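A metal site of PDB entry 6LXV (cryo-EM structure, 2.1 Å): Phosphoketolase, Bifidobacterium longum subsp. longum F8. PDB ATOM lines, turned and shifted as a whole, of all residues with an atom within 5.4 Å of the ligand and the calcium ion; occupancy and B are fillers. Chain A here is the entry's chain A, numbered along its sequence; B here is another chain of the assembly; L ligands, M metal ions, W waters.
A nitrogen (N3) of the ligand is in hydrogen-bond range of the backbone carbonyl oxygen of Gly 155 (2.9 Å). The backbone NH of Leu 157 lies within hydrogen-bond range of a nitrogen (N2) of the ligand (3.2 Å). A nitrogen (N1) of the ligand is in hydrogen-bond range of the side-chain carboxylate of Glu 479 of chain B, 2.7 Å away. O2 of the ligand lies within hydrogen-bond range of N of Gly 183. An oxygen (O7) of the ligand is in hydrogen-bond range of a ring nitrogen (NE2) of His 97, 2.6 Å away. An oxygen (O6) of the ligand sits at hydrogen-bond distance from the side-chain hydroxyl (OG1) of Thr 67, 2.9 Å away. A sulfur (S1) of the ligand sits close to a ring nitrogen (NE2) of His 320. NZ of Lys 300 is in salt-bridge range of O7 of the ligand (3.5 Å). The backbone NH (N) of Glu 184 is in hydrogen-bond range of an oxygen (O2) of the ligand.
The backbone NH of Gly 66 is in hydrogen-bond range of the backbone carbonyl oxygen of His 320 (3.2 Å). The side-chain hydroxyl (OG1) of Thr 187 lies within hydrogen-bond range of the backbone carbonyl oxygen (O) of Glu 184 (3.0 Å). OG1 of Thr 67 lies close to NE2 of His 213. N of Ile 219 lies within hydrogen-bond range of OD2 of Asp 436 of chain B. A ring nitrogen (ND1) of His 320 lies within hydrogen-bond range of the side-chain amino group of Lys 300 (3.0 Å). N of Asp 182 is in hydrogen-bond range of O of His 213 (3.4 Å). The side-chain amino group (NZ) of Lys 300 sits at hydrogen-bond distance from the backbone carbonyl oxygen (O) of Lys 218 (3.0 Å). OE1 of Glu 184 is in hydrogen-bond range of N of Gly 181 (3.2 Å).
CB of Pro 95 touches O6 of the ligand, 3.7 Å away. Glu 156 touches the ligand (CA to N2, 3.9 Å). CA of Gly 181 touches O2 of the ligand, at 3.2 Å. His 213 touches the ligand (CD2 to O6, 3.7 Å). CB of Lys 218 touches O1 of the ligand, 3.7 Å away. Ile 219 touches the ligand. OD2 of Asp 436 of chain B touches C10 of the ligand (3.6 Å). OE2 of Glu 437 of chain B touches C5 of the ligand, 3.2 Å away. Leu 477 of chain B touches the ligand. CE2 of Phe 504 of chain B touches C4 of the ligand, 3.4 Å away. Hydrophobic or aromatic side chains that line the ligand: Pro 95, His 97, Leu 157, His 213, Ile 219, His 320, Leu 477 of chain B and Phe 504 of chain B. The nearest printed residue that does not touch the ligand is Tyr 501 of chain B (4.3 Å).
Of the 31 residues printed, 3 come within 4 Å of the calcium ion.
O of Tyr 217 is bound to the calcium ion (2.2 Å). The side-chain carboxylate (OD1) of Asp 182 is bound to the calcium ion, 2.3 Å away. OD1 of Asn 215 binds the calcium ion, 2.3 Å away. O5 of the ligand binds the calcium ion (2.3 Å). The calcium ion is bound by O3 of the ligand (2.3 Å). Water W4 is bound to the calcium ion. The calcium ion has six donor atoms within binding distance.
Water W4 lies within hydrogen-bond range of O6 of the ligand, O of His 213, N of Asp 182 and ND2 of Asn 215. Water W2 lies within hydrogen-bond range of an oxygen (O7) of the ligand (2.9 Å), the backbone carbonyl oxygen of His 320 (3.0 Å), the backbone NH of Thr 67 (3.0 Å), a ring nitrogen (NE2) of His 97 (3.3 Å) and the backbone NH of Gly 66 (3.4 Å). Water W1 lies within hydrogen-bond range of NE2 of His 553 of chain B (2.4 Å), O of Gly 155 (3.0 Å) and N3 of the ligand (3.4 Å). Water W3 lies within hydrogen-bond range of O of Gly 155 (3.0 Å), ND1 of His 97 (3.0 Å) and N3 of the ligand (3.5 Å).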
ATOM      1  N   GLY A  66     -19.434  17.733  21.960  1.00  0.00           N
ATOM      2  CA  GLY A  66     -18.245  17.810  21.123  1.00  0.00           C
ATOM      3  C   GLY A  66     -18.394  17.183  19.749  1.00  0.00           C
ATOM      4  O   GLY A  66     -18.237  17.848  18.746  1.00  0.00           O
ATOM      5  N   THR A  67     -18.889  15.968  19.700  1.00  0.00           N
ATOM      6  CA  THR A  67     -19.165  15.311  18.437  1.00  0.00           C
ATOM      7  C   THR A  67     -20.387  15.887  17.689  1.00  0.00           C
ATOM      8  O   THR A  67     -20.430  15.761  16.492  1.00  0.00           O
ATOM      9  CB  THR A  67     -19.334  13.802  18.701  1.00  0.00           C
ATOM     10  OG1 THR A  67     -19.302  13.111  17.474  1.00  0.00           O
ATOM     11  CG2 THR A  67     -20.635  13.478  19.414  1.00  0.00           C
ATOM     12  N   PRO A  95     -20.068   7.606  17.051  1.00  0.00           N
ATOM     13  CA  PRO A  95     -20.041   8.374  18.318  1.00  0.00           C
ATOM     14  C   PRO A  95     -21.456   8.543  18.855  1.00  0.00           C
ATOM     15  O   PRO A  95     -22.084   9.546  18.737  1.00  0.00           O
ATOM     16  CB  PRO A  95     -19.415   9.706  17.888  1.00  0.00           C
ATOM     17  CG  PRO A  95     -18.991   9.518  16.515  1.00  0.00           C
ATOM     18  CD  PRO A  95     -19.884   8.531  15.943  1.00  0.00           C
ATOM     19  N   HIS A  97     -22.843   8.776  21.677  1.00  0.00           N
ATOM     20  CA  HIS A  97     -23.055   9.849  22.615  1.00  0.00           C
ATOM     21  C   HIS A  97     -23.411  11.172  21.944  1.00  0.00           C
ATOM     22  O   HIS A  97     -23.735  12.100  22.656  1.00  0.00           O
ATOM     23  CB  HIS A  97     -21.827  10.051  23.491  1.00  0.00           C
ATOM     24  CG  HIS A  97     -20.572  10.329  22.725  1.00  0.00           C
ATOM     25  ND1 HIS A  97     -19.888   9.378  22.022  1.00  0.00           N
ATOM     26  CD2 HIS A  97     -19.912  11.487  22.511  1.00  0.00           C
ATOM     27  CE1 HIS A  97     -18.844   9.920  21.455  1.00  0.00           C
ATOM     28  NE2 HIS A  97     -18.826  11.188  21.747  1.00  0.00           N
ATOM     29  N   GLY A 155     -22.827   3.310  22.423  1.00  0.00           N
ATOM     30  CA  GLY A 155     -22.430   3.645  23.775  1.00  0.00           C
ATOM     31  C   GLY A 155     -21.056   3.101  24.064  1.00  0.00           C
ATOM     32  O   GLY A 155     -20.095   3.831  24.219  1.00  0.00           O
ATOM     33  N   GLU A 156     -20.961   1.803  24.037  1.00  0.00           N
ATOM     34  CA  GLU A 156     -19.685   1.137  23.967  1.00  0.00           C
ATOM     35  C   GLU A 156     -19.089   1.243  22.559  1.00  0.00           C
ATOM     36  O   GLU A 156     -19.681   0.795  21.607  1.00  0.00           O
ATOM     37  CB  GLU A 156     -19.865  -0.311  24.346  1.00  0.00           C
ATOM     38  CG  GLU A 156     -18.654  -1.043  24.589  1.00  0.00           C
ATOM     39  CD  GLU A 156     -18.967  -2.376  25.179  1.00  0.00           C
ATOM     40  OE1 GLU A 156     -19.625  -2.417  26.217  1.00  0.00           O
ATOM     41  OE2 GLU A 156     -18.596  -3.380  24.561  1.00  0.00           O
ATOM     42  N   LEU A 157     -17.886   1.734  22.469  1.00  0.00           N
ATOM     43  CA  LEU A 157     -17.336   2.125  21.170  1.00  0.00           C
ATOM     44  C   LEU A 157     -16.575   1.009  20.481  1.00  0.00           C
ATOM     45  O   LEU A 157     -16.024   0.134  21.123  1.00  0.00           O
ATOM     46  CB  LEU A 157     -16.446   3.330  21.374  1.00  0.00           C
ATOM     47  CG  LEU A 157     -17.159   4.596  21.809  1.00  0.00           C
ATOM     48  CD1 LEU A 157     -16.103   5.601  22.130  1.00  0.00           C
ATOM     49  CD2 LEU A 157     -18.110   5.139  20.788  1.00  0.00           C
ATOM     50  N   GLY A 181     -15.962   7.671  15.186  1.00  0.00           N
ATOM     51  CA  GLY A 181     -15.146   8.463  16.098  1.00  0.00           C
ATOM     52  C   GLY A 181     -13.643   8.357  15.897  1.00  0.00           C
ATOM     53  O   GLY A 181     -13.211   7.273  15.600  1.00  0.00           O
ATOM     54  N   ASP A 182     -12.847   9.411  15.988  1.00  0.00           N
ATOM     55  CA  ASP A 182     -11.433   9.146  15.827  1.00  0.00           C
ATOM     56  C   ASP A 182     -10.814   8.542  17.085  1.00  0.00           C
ATOM     57  O   ASP A 182      -9.863   7.814  16.969  1.00  0.00           O
ATOM     58  CB  ASP A 182     -10.623  10.363  15.338  1.00  0.00           C
ATOM     59  CG  ASP A 182     -10.694  11.605  16.208  1.00  0.00           C
ATOM     60  OD1 ASP A 182     -11.458  11.678  17.045  1.00  0.00           O
ATOM     61  OD2 ASP A 182      -9.930  12.513  16.059  1.00  0.00           O
ATOM     62  N   GLY A 183     -11.413   8.778  18.243  1.00  0.00           N
ATOM     63  CA  GLY A 183     -11.129   7.997  19.414  1.00  0.00           C
ATOM     64  C   GLY A 183     -11.621   6.572  19.295  1.00  0.00           C
ATOM     65  O   GLY A 183     -10.904   5.654  19.605  1.00  0.00           O
ATOM     66  N   GLU A 184     -12.813   6.386  18.774  1.00  0.00           N
ATOM     67  CA  GLU A 184     -13.352   5.054  18.558  1.00  0.00           C
ATOM     68  C   GLU A 184     -12.476   4.217  17.623  1.00  0.00           C
ATOM     69  O   GLU A 184     -12.342   3.029  17.808  1.00  0.00           O
ATOM     70  CB  GLU A 184     -14.773   5.147  17.999  1.00  0.00           C
ATOM     71  CG  GLU A 184     -15.389   3.806  17.509  1.00  0.00           C
ATOM     72  CD  GLU A 184     -16.835   3.919  16.958  1.00  0.00           C
ATOM     73  OE1 GLU A 184     -17.212   4.962  16.411  1.00  0.00           O
ATOM     74  OE2 GLU A 184     -17.585   2.969  17.081  1.00  0.00           O
ATOM     75  N   ALA A 185     -11.838   4.840  16.644  1.00  0.00           N
ATOM     76  CA  ALA A 185     -10.875   4.173  15.804  1.00  0.00           C
ATOM     77  C   ALA A 185      -9.624   3.644  16.529  1.00  0.00           C
ATOM     78  O   ALA A 185      -8.934   2.809  15.983  1.00  0.00           O
ATOM     79  CB  ALA A 185     -10.486   5.103  14.699  1.00  0.00           C
ATOM     80  N   THR A 187      -9.986   1.712  19.186  1.00  0.00           N
ATOM     81  CA  THR A 187     -10.329   0.465  19.841  1.00  0.00           C
ATOM     82  C   THR A 187      -9.931  -0.737  18.992  1.00  0.00           C
ATOM     83  O   THR A 187      -9.728  -0.648  17.793  1.00  0.00           O
ATOM     84  CB  THR A 187     -11.817   0.349  20.194  1.00  0.00           C
ATOM     85  OG1 THR A 187     -12.599   0.253  19.009  1.00  0.00           O
ATOM     86  CG2 THR A 187     -12.323   1.458  21.002  1.00  0.00           C
ATOM     87  N   HIS A 213     -14.654  10.630  11.702  1.00  0.00           N
ATOM     88  CA  HIS A 213     -14.960  11.900  12.384  1.00  0.00           C
ATOM     89  C   HIS A 213     -13.715  12.391  13.126  1.00  0.00           C
ATOM     90  O   HIS A 213     -13.598  12.328  14.335  1.00  0.00           O
ATOM     91  CB  HIS A 213     -16.155  11.667  13.291  1.00  0.00           C
ATOM     92  CG  HIS A 213     -16.775  12.900  13.858  1.00  0.00           C
ATOM     93  ND1 HIS A 213     -16.431  14.180  13.494  1.00  0.00           N
ATOM     94  CD2 HIS A 213     -17.717  13.027  14.804  1.00  0.00           C
ATOM     95  CE1 HIS A 213     -17.170  15.024  14.157  1.00  0.00           C
ATOM     96  NE2 HIS A 213     -17.964  14.351  14.957  1.00  0.00           N
ATOM     97  N   ASN A 215     -12.082  14.702  14.596  1.00  0.00           N
ATOM     98  CA  ASN A 215     -12.191  16.000  15.225  1.00  0.00           C
ATOM     99  C   ASN A 215     -10.992  16.272  16.120  1.00  0.00           C
ATOM    100  O   ASN A 215     -10.945  17.280  16.747  1.00  0.00           O
ATOM    101  CB  ASN A 215     -13.574  16.194  15.912  1.00  0.00           C
ATOM    102  CG  ASN A 215     -13.896  15.192  16.995  1.00  0.00           C
ATOM    103  OD1 ASN A 215     -13.041  14.588  17.468  1.00  0.00           O
ATOM    104  ND2 ASN A 215     -15.126  14.977  17.292  1.00  0.00           N
ATOM    105  N   GLY A 216     -10.062  15.350  16.226  1.00  0.00           N
ATOM    106  CA  GLY A 216      -8.809  15.561  16.877  1.00  0.00           C
ATOM    107  C   GLY A 216      -8.687  15.095  18.305  1.00  0.00           C
ATOM    108  O   GLY A 216      -7.604  15.073  18.803  1.00  0.00           O
ATOM    109  N   TYR A 217      -9.795  14.779  18.977  1.00  0.00           N
ATOM    110  CA  TYR A 217      -9.912  14.634  20.422  1.00  0.00           C
ATOM    111  C   TYR A 217     -10.914  13.533  20.708  1.00  0.00           C
ATOM    112  O   TYR A 217     -11.796  13.252  19.933  1.00  0.00           O
ATOM    113  CB  TYR A 217     -10.231  15.971  21.198  1.00  0.00           C
ATOM    114  CG  TYR A 217      -9.148  16.949  20.990  1.00  0.00           C
ATOM    115  CD1 TYR A 217      -9.267  17.866  19.957  1.00  0.00           C
ATOM    116  CD2 TYR A 217      -7.951  16.901  21.714  1.00  0.00           C
ATOM    117  CE1 TYR A 217      -8.313  18.612  19.635  1.00  0.00           C
ATOM    118  CE2 TYR A 217      -6.976  17.713  21.402  1.00  0.00           C
ATOM    119  CZ  TYR A 217      -7.158  18.578  20.367  1.00  0.00           C
ATOM    120  OH  TYR A 217      -6.236  19.429  19.976  1.00  0.00           O
ATOM    121  N   LYS A 218     -10.694  12.863  21.806  1.00  0.00           N
ATOM    122  CA  LYS A 218     -11.537  11.954  22.515  1.00  0.00           C
ATOM    123  C   LYS A 218     -11.887  12.702  23.816  1.00  0.00           C
ATOM    124  O   LYS A 218     -12.182  13.893  23.725  1.00  0.00           O
ATOM    125  CB  LYS A 218     -10.869  10.587  22.622  1.00  0.00           C
ATOM    126  CG  LYS A 218      -9.462  10.470  23.068  1.00  0.00           C
ATOM    127  CD  LYS A 218      -9.026   8.998  23.139  1.00  0.00           C
ATOM    128  CE  LYS A 218      -7.618   8.857  23.664  1.00  0.00           C
ATOM    129  NZ  LYS A 218      -6.547   9.168  22.772  1.00  0.00           N
ATOM    130  N   ILE A 219     -12.097  12.023  24.934  1.00  0.00           N
ATOM    131  CA  ILE A 219     -12.604  12.699  26.149  1.00  0.00           C
ATOM    132  C   ILE A 219     -11.649  13.780  26.641  1.00  0.00           C
ATOM    133  O   ILE A 219     -12.029  14.916  26.829  1.00  0.00           O
ATOM    134  CB  ILE A 219     -12.906  11.726  27.286  1.00  0.00           C
ATOM    135  CG1 ILE A 219     -14.033  10.770  26.933  1.00  0.00           C
ATOM    136  CG2 ILE A 219     -13.207  12.507  28.584  1.00  0.00           C
ATOM    137  CD1 ILE A 219     -14.363   9.946  27.962  1.00  0.00           C
ATOM    138  N   THR A 223      -6.249  12.430  19.608  1.00  0.00           N
ATOM    139  CA  THR A 223      -6.414  11.132  19.012  1.00  0.00           C
ATOM    140  C   THR A 223      -5.175  10.831  18.189  1.00  0.00           C
ATOM    141  O   THR A 223      -4.644  11.721  17.557  1.00  0.00           O
ATOM    142  CB  THR A 223      -7.737  11.049  18.203  1.00  0.00           C
ATOM    143  OG1 THR A 223      -7.828  12.099  17.245  1.00  0.00           O
ATOM    144  CG2 THR A 223      -8.974  11.076  19.129  1.00  0.00           C
ATOM    145  N   LYS A 300     -13.371  19.984  17.108  1.00  0.00           N
ATOM    146  CA  LYS A 300     -14.295  19.367  18.037  1.00  0.00           C
ATOM    147  C   LYS A 300     -15.166  20.430  18.705  1.00  0.00           C
ATOM    148  O   LYS A 300     -14.688  21.495  19.040  1.00  0.00           O
ATOM    149  CB  LYS A 300     -13.578  18.513  19.082  1.00  0.00           C
ATOM    150  CG  LYS A 300     -14.512  17.696  19.872  1.00  0.00           C
ATOM    151  CD  LYS A 300     -13.869  16.761  20.776  1.00  0.00           C
ATOM    152  CE  LYS A 300     -14.856  15.856  21.369  1.00  0.00           C
ATOM    153  NZ  LYS A 300     -14.345  14.579  21.812  1.00  0.00           N
ATOM    154  N   HIS A 320     -15.960  18.231  24.905  1.00  0.00           N
ATOM    155  CA  HIS A 320     -16.452  16.863  24.752  1.00  0.00           C
ATOM    156  C   HIS A 320     -17.832  16.659  25.373  1.00  0.00           C
ATOM    157  O   HIS A 320     -18.775  16.260  24.705  1.00  0.00           O
ATOM    158  CB  HIS A 320     -15.485  15.851  25.353  1.00  0.00           C
ATOM    159  CG  HIS A 320     -16.001  14.455  25.312  1.00  0.00           C
ATOM    160  ND1 HIS A 320     -16.122  13.765  24.144  1.00  0.00           N
ATOM    161  CD2 HIS A 320     -16.556  13.692  26.256  1.00  0.00           C
ATOM    162  CE1 HIS A 320     -16.661  12.591  24.387  1.00  0.00           C
ATOM    163  NE2 HIS A 320     -16.901  12.516  25.675  1.00  0.00           N
ATOM    164  N   PRO B 435      -8.087   3.918  29.715  1.00  0.00           N
ATOM    165  CA  PRO B 435      -8.573   4.173  28.372  1.00  0.00           C
ATOM    166  C   PRO B 435      -9.218   5.547  28.244  1.00  0.00           C
ATOM    167  O   PRO B 435     -10.402   5.650  28.076  1.00  0.00           O
ATOM    168  CB  PRO B 435      -9.552   3.036  28.159  1.00  0.00           C
ATOM    169  CG  PRO B 435     -10.039   2.769  29.473  1.00  0.00           C
ATOM    170  CD  PRO B 435      -8.952   2.950  30.392  1.00  0.00           C
ATOM    171  N   ASP B 436      -8.388   6.591  28.325  1.00  0.00           N
ATOM    172  CA  ASP B 436      -8.787   8.008  28.247  1.00  0.00           C
ATOM    173  C   ASP B 436      -9.723   8.344  29.425  1.00  0.00           C
ATOM    174  O   ASP B 436     -10.665   9.096  29.325  1.00  0.00           O
ATOM    175  CB  ASP B 436      -9.336   8.273  26.830  1.00  0.00           C
ATOM    176  CG  ASP B 436      -9.795   9.681  26.567  1.00  0.00           C
ATOM    177  OD1 ASP B 436      -9.127  10.710  26.796  1.00  0.00           O
ATOM    178  OD2 ASP B 436     -10.882   9.673  26.091  1.00  0.00           O
ATOM    179  N   GLU B 437      -9.481   7.713  30.544  1.00  0.00           N
ATOM    180  CA  GLU B 437     -10.364   7.850  31.690  1.00  0.00           C
ATOM    181  C   GLU B 437      -9.639   8.169  32.995  1.00  0.00           C
ATOM    182  O   GLU B 437     -10.287   8.170  34.011  1.00  0.00           O
ATOM    183  CB  GLU B 437     -11.226   6.571  31.854  1.00  0.00           C
ATOM    184  CG  GLU B 437     -12.351   6.421  30.823  1.00  0.00           C
ATOM    185  CD  GLU B 437     -12.929   5.011  30.736  1.00  0.00           C
ATOM    186  OE1 GLU B 437     -12.724   4.231  31.623  1.00  0.00           O
ATOM    187  OE2 GLU B 437     -13.596   4.661  29.762  1.00  0.00           O
ATOM    188  N   LEU B 477      -7.549   4.849  23.864  1.00  0.00           N
ATOM    189  CA  LEU B 477      -8.917   4.381  23.977  1.00  0.00           C
ATOM    190  C   LEU B 477      -9.031   2.937  23.454  1.00  0.00           C
ATOM    191  O   LEU B 477      -9.461   2.672  22.338  1.00  0.00           O
ATOM    192  CB  LEU B 477      -9.855   5.348  23.279  1.00  0.00           C
ATOM    193  CG  LEU B 477     -11.356   5.079  23.141  1.00  0.00           C
ATOM    194  CD1 LEU B 477     -11.982   4.412  24.246  1.00  0.00           C
ATOM    195  CD2 LEU B 477     -12.149   6.206  22.582  1.00  0.00           C
ATOM    196  N   GLU B 479      -9.378  -0.707  25.956  1.00  0.00           N
ATOM    197  CA  GLU B 479      -9.232  -1.532  27.145  1.00  0.00           C
ATOM    198  C   GLU B 479      -8.277  -2.695  26.907  1.00  0.00           C
ATOM    199  O   GLU B 479      -7.487  -2.994  27.772  1.00  0.00           O
ATOM    200  CB  GLU B 479     -10.612  -2.007  27.637  1.00  0.00           C
ATOM    201  CG  GLU B 479     -11.639  -0.953  28.097  1.00  0.00           C
ATOM    202  CD  GLU B 479     -12.278  -0.059  27.006  1.00  0.00           C
ATOM    203  OE1 GLU B 479     -12.339  -0.409  25.835  1.00  0.00           O
ATOM    204  OE2 GLU B 479     -12.720   1.031  27.352  1.00  0.00           O
ATOM    205  N   TYR B 501     -14.118   2.606  33.550  1.00  0.00           N
ATOM    206  CA  TYR B 501     -15.520   2.564  33.880  1.00  0.00           C
ATOM    207  C   TYR B 501     -15.929   1.126  33.990  1.00  0.00           C
ATOM    208  O   TYR B 501     -15.469   0.290  33.205  1.00  0.00           O
ATOM    209  CB  TYR B 501     -16.380   3.240  32.832  1.00  0.00           C
ATOM    210  CG  TYR B 501     -16.099   4.665  32.582  1.00  0.00           C
ATOM    211  CD1 TYR B 501     -15.379   5.456  33.472  1.00  0.00           C
ATOM    212  CD2 TYR B 501     -16.528   5.237  31.429  1.00  0.00           C
ATOM    213  CE1 TYR B 501     -15.136   6.701  33.207  1.00  0.00           C
ATOM    214  CE2 TYR B 501     -16.303   6.504  31.151  1.00  0.00           C
ATOM    215  CZ  TYR B 501     -15.609   7.241  32.035  1.00  0.00           C
ATOM    216  OH  TYR B 501     -15.385   8.512  31.720  1.00  0.00           O
ATOM    217  N   PHE B 504     -17.360  -1.073  31.046  1.00  0.00           N
ATOM    218  CA  PHE B 504     -16.412  -1.416  30.002  1.00  0.00           C
ATOM    219  C   PHE B 504     -15.315  -2.353  30.454  1.00  0.00           C
ATOM    220  O   PHE B 504     -14.499  -2.715  29.628  1.00  0.00           O
ATOM    221  CB  PHE B 504     -15.782  -0.182  29.420  1.00  0.00           C
ATOM    222  CG  PHE B 504     -16.755   0.841  28.925  1.00  0.00           C
ATOM    223  CD1 PHE B 504     -17.811   0.502  28.123  1.00  0.00           C
ATOM    224  CD2 PHE B 504     -16.580   2.168  29.218  1.00  0.00           C
ATOM    225  CE1 PHE B 504     -18.695   1.471  27.670  1.00  0.00           C
ATOM    226  CE2 PHE B 504     -17.455   3.095  28.759  1.00  0.00           C
ATOM    227  CZ  PHE B 504     -18.488   2.755  27.961  1.00  0.00           C
ATOM    228  N   VAL B 507     -15.263  -5.553  28.251  1.00  0.00           N
ATOM    229  CA  VAL B 507     -14.401  -5.552  27.088  1.00  0.00           C
ATOM    230  C   VAL B 507     -13.197  -6.462  27.246  1.00  0.00           C
ATOM    231  O   VAL B 507     -12.831  -7.132  26.307  1.00  0.00           O
ATOM    232  CB  VAL B 507     -13.994  -4.110  26.694  1.00  0.00           C
ATOM    233  CG1 VAL B 507     -13.070  -4.108  25.493  1.00  0.00           C
ATOM    234  CG2 VAL B 507     -15.235  -3.267  26.439  1.00  0.00           C
ATOM    235  N   HIS B 553     -25.014   1.738  29.701  1.00  0.00           N
ATOM    236  CA  HIS B 553     -23.728   1.812  30.378  1.00  0.00           C
ATOM    237  C   HIS B 553     -23.777   1.239  31.771  1.00  0.00           C
ATOM    238  O   HIS B 553     -22.856   1.435  32.540  1.00  0.00           O
ATOM    239  CB  HIS B 553     -23.257   3.228  30.505  1.00  0.00           C
ATOM    240  CG  HIS B 553     -22.953   3.888  29.204  1.00  0.00           C
ATOM    241  ND1 HIS B 553     -23.930   4.208  28.295  1.00  0.00           N
ATOM    242  CD2 HIS B 553     -21.806   4.391  28.720  1.00  0.00           C
ATOM    243  CE1 HIS B 553     -23.374   4.804  27.264  1.00  0.00           C
ATOM    244  NE2 HIS B 553     -22.082   4.905  27.492  1.00  0.00           N
HETATM  245  N1  LIG L   1     -14.462   2.778  26.242  1.00  0.00           N
HETATM  246  C1  LIG L   1     -15.358   2.231  25.356  1.00  0.00           C
HETATM  247  C2  LIG L   1     -15.210   0.847  24.771  1.00  0.00           C
HETATM  248  N2  LIG L   1     -16.404   3.022  24.977  1.00  0.00           N
HETATM  249  C3  LIG L   1     -16.568   4.278  25.458  1.00  0.00           C
HETATM  250  N3  LIG L   1     -17.607   4.935  25.116  1.00  0.00           N
HETATM  251  C4  LIG L   1     -15.685   4.806  26.391  1.00  0.00           C
HETATM  252  C5  LIG L   1     -14.617   4.021  26.748  1.00  0.00           C
HETATM  253  C6  LIG L   1     -15.856   6.192  26.922  1.00  0.00           C
HETATM  254  N4  LIG L   1     -15.922   7.222  25.906  1.00  0.00           N
HETATM  255  C7  LIG L   1     -17.022   7.874  25.392  1.00  0.00           C
HETATM  256  S1  LIG L   1     -16.897   9.013  24.334  1.00  0.00           S
HETATM  257  C8  LIG L   1     -15.344   8.677  24.420  1.00  0.00           C
HETATM  258  C9  LIG L   1     -14.922   7.699  25.276  1.00  0.00           C
HETATM  259  C10 LIG L   1     -13.524   7.338  25.601  1.00  0.00           C
HETATM  260  C11 LIG L   1     -14.528   9.495  23.503  1.00  0.00           C
HETATM  261  C12 LIG L   1     -14.961   9.123  22.134  1.00  0.00           C
HETATM  262  O1  LIG L   1     -14.130   9.638  21.132  1.00  0.00           O
HETATM  263  P1  LIG L   1     -14.439   9.809  19.649  1.00  0.00           P
HETATM  264  O2  LIG L   1     -14.465   8.424  19.251  1.00  0.00           O
HETATM  265  O3  LIG L   1     -13.191  10.407  19.488  1.00  0.00           O
HETATM  266  O4  LIG L   1     -15.763  10.595  19.856  1.00  0.00           O
HETATM  267  P2  LIG L   1     -16.205  12.062  19.596  1.00  0.00           P
HETATM  268  O5  LIG L   1     -15.113  12.868  19.601  1.00  0.00           O
HETATM  269  O6  LIG L   1     -16.648  12.205  18.259  1.00  0.00           O
HETATM  270  O7  LIG L   1     -16.975  12.679  20.625  1.00  0.00           O
HETATM  271 CA    CA M   1     -13.187  12.462  18.356  1.00  0.00          CA
HETATM  272  O   HOH W   1     -20.573   6.184  26.066  1.00  0.00           O
HETATM  273  O   HOH W   2     -18.442  14.464  22.294  1.00  0.00           O
HETATM  274  O   HOH W   3     -20.019   6.690  23.376  1.00  0.00           O
HETATM  275  O   HOH W   4     -14.707  11.625  16.698  1.00  0.00           O
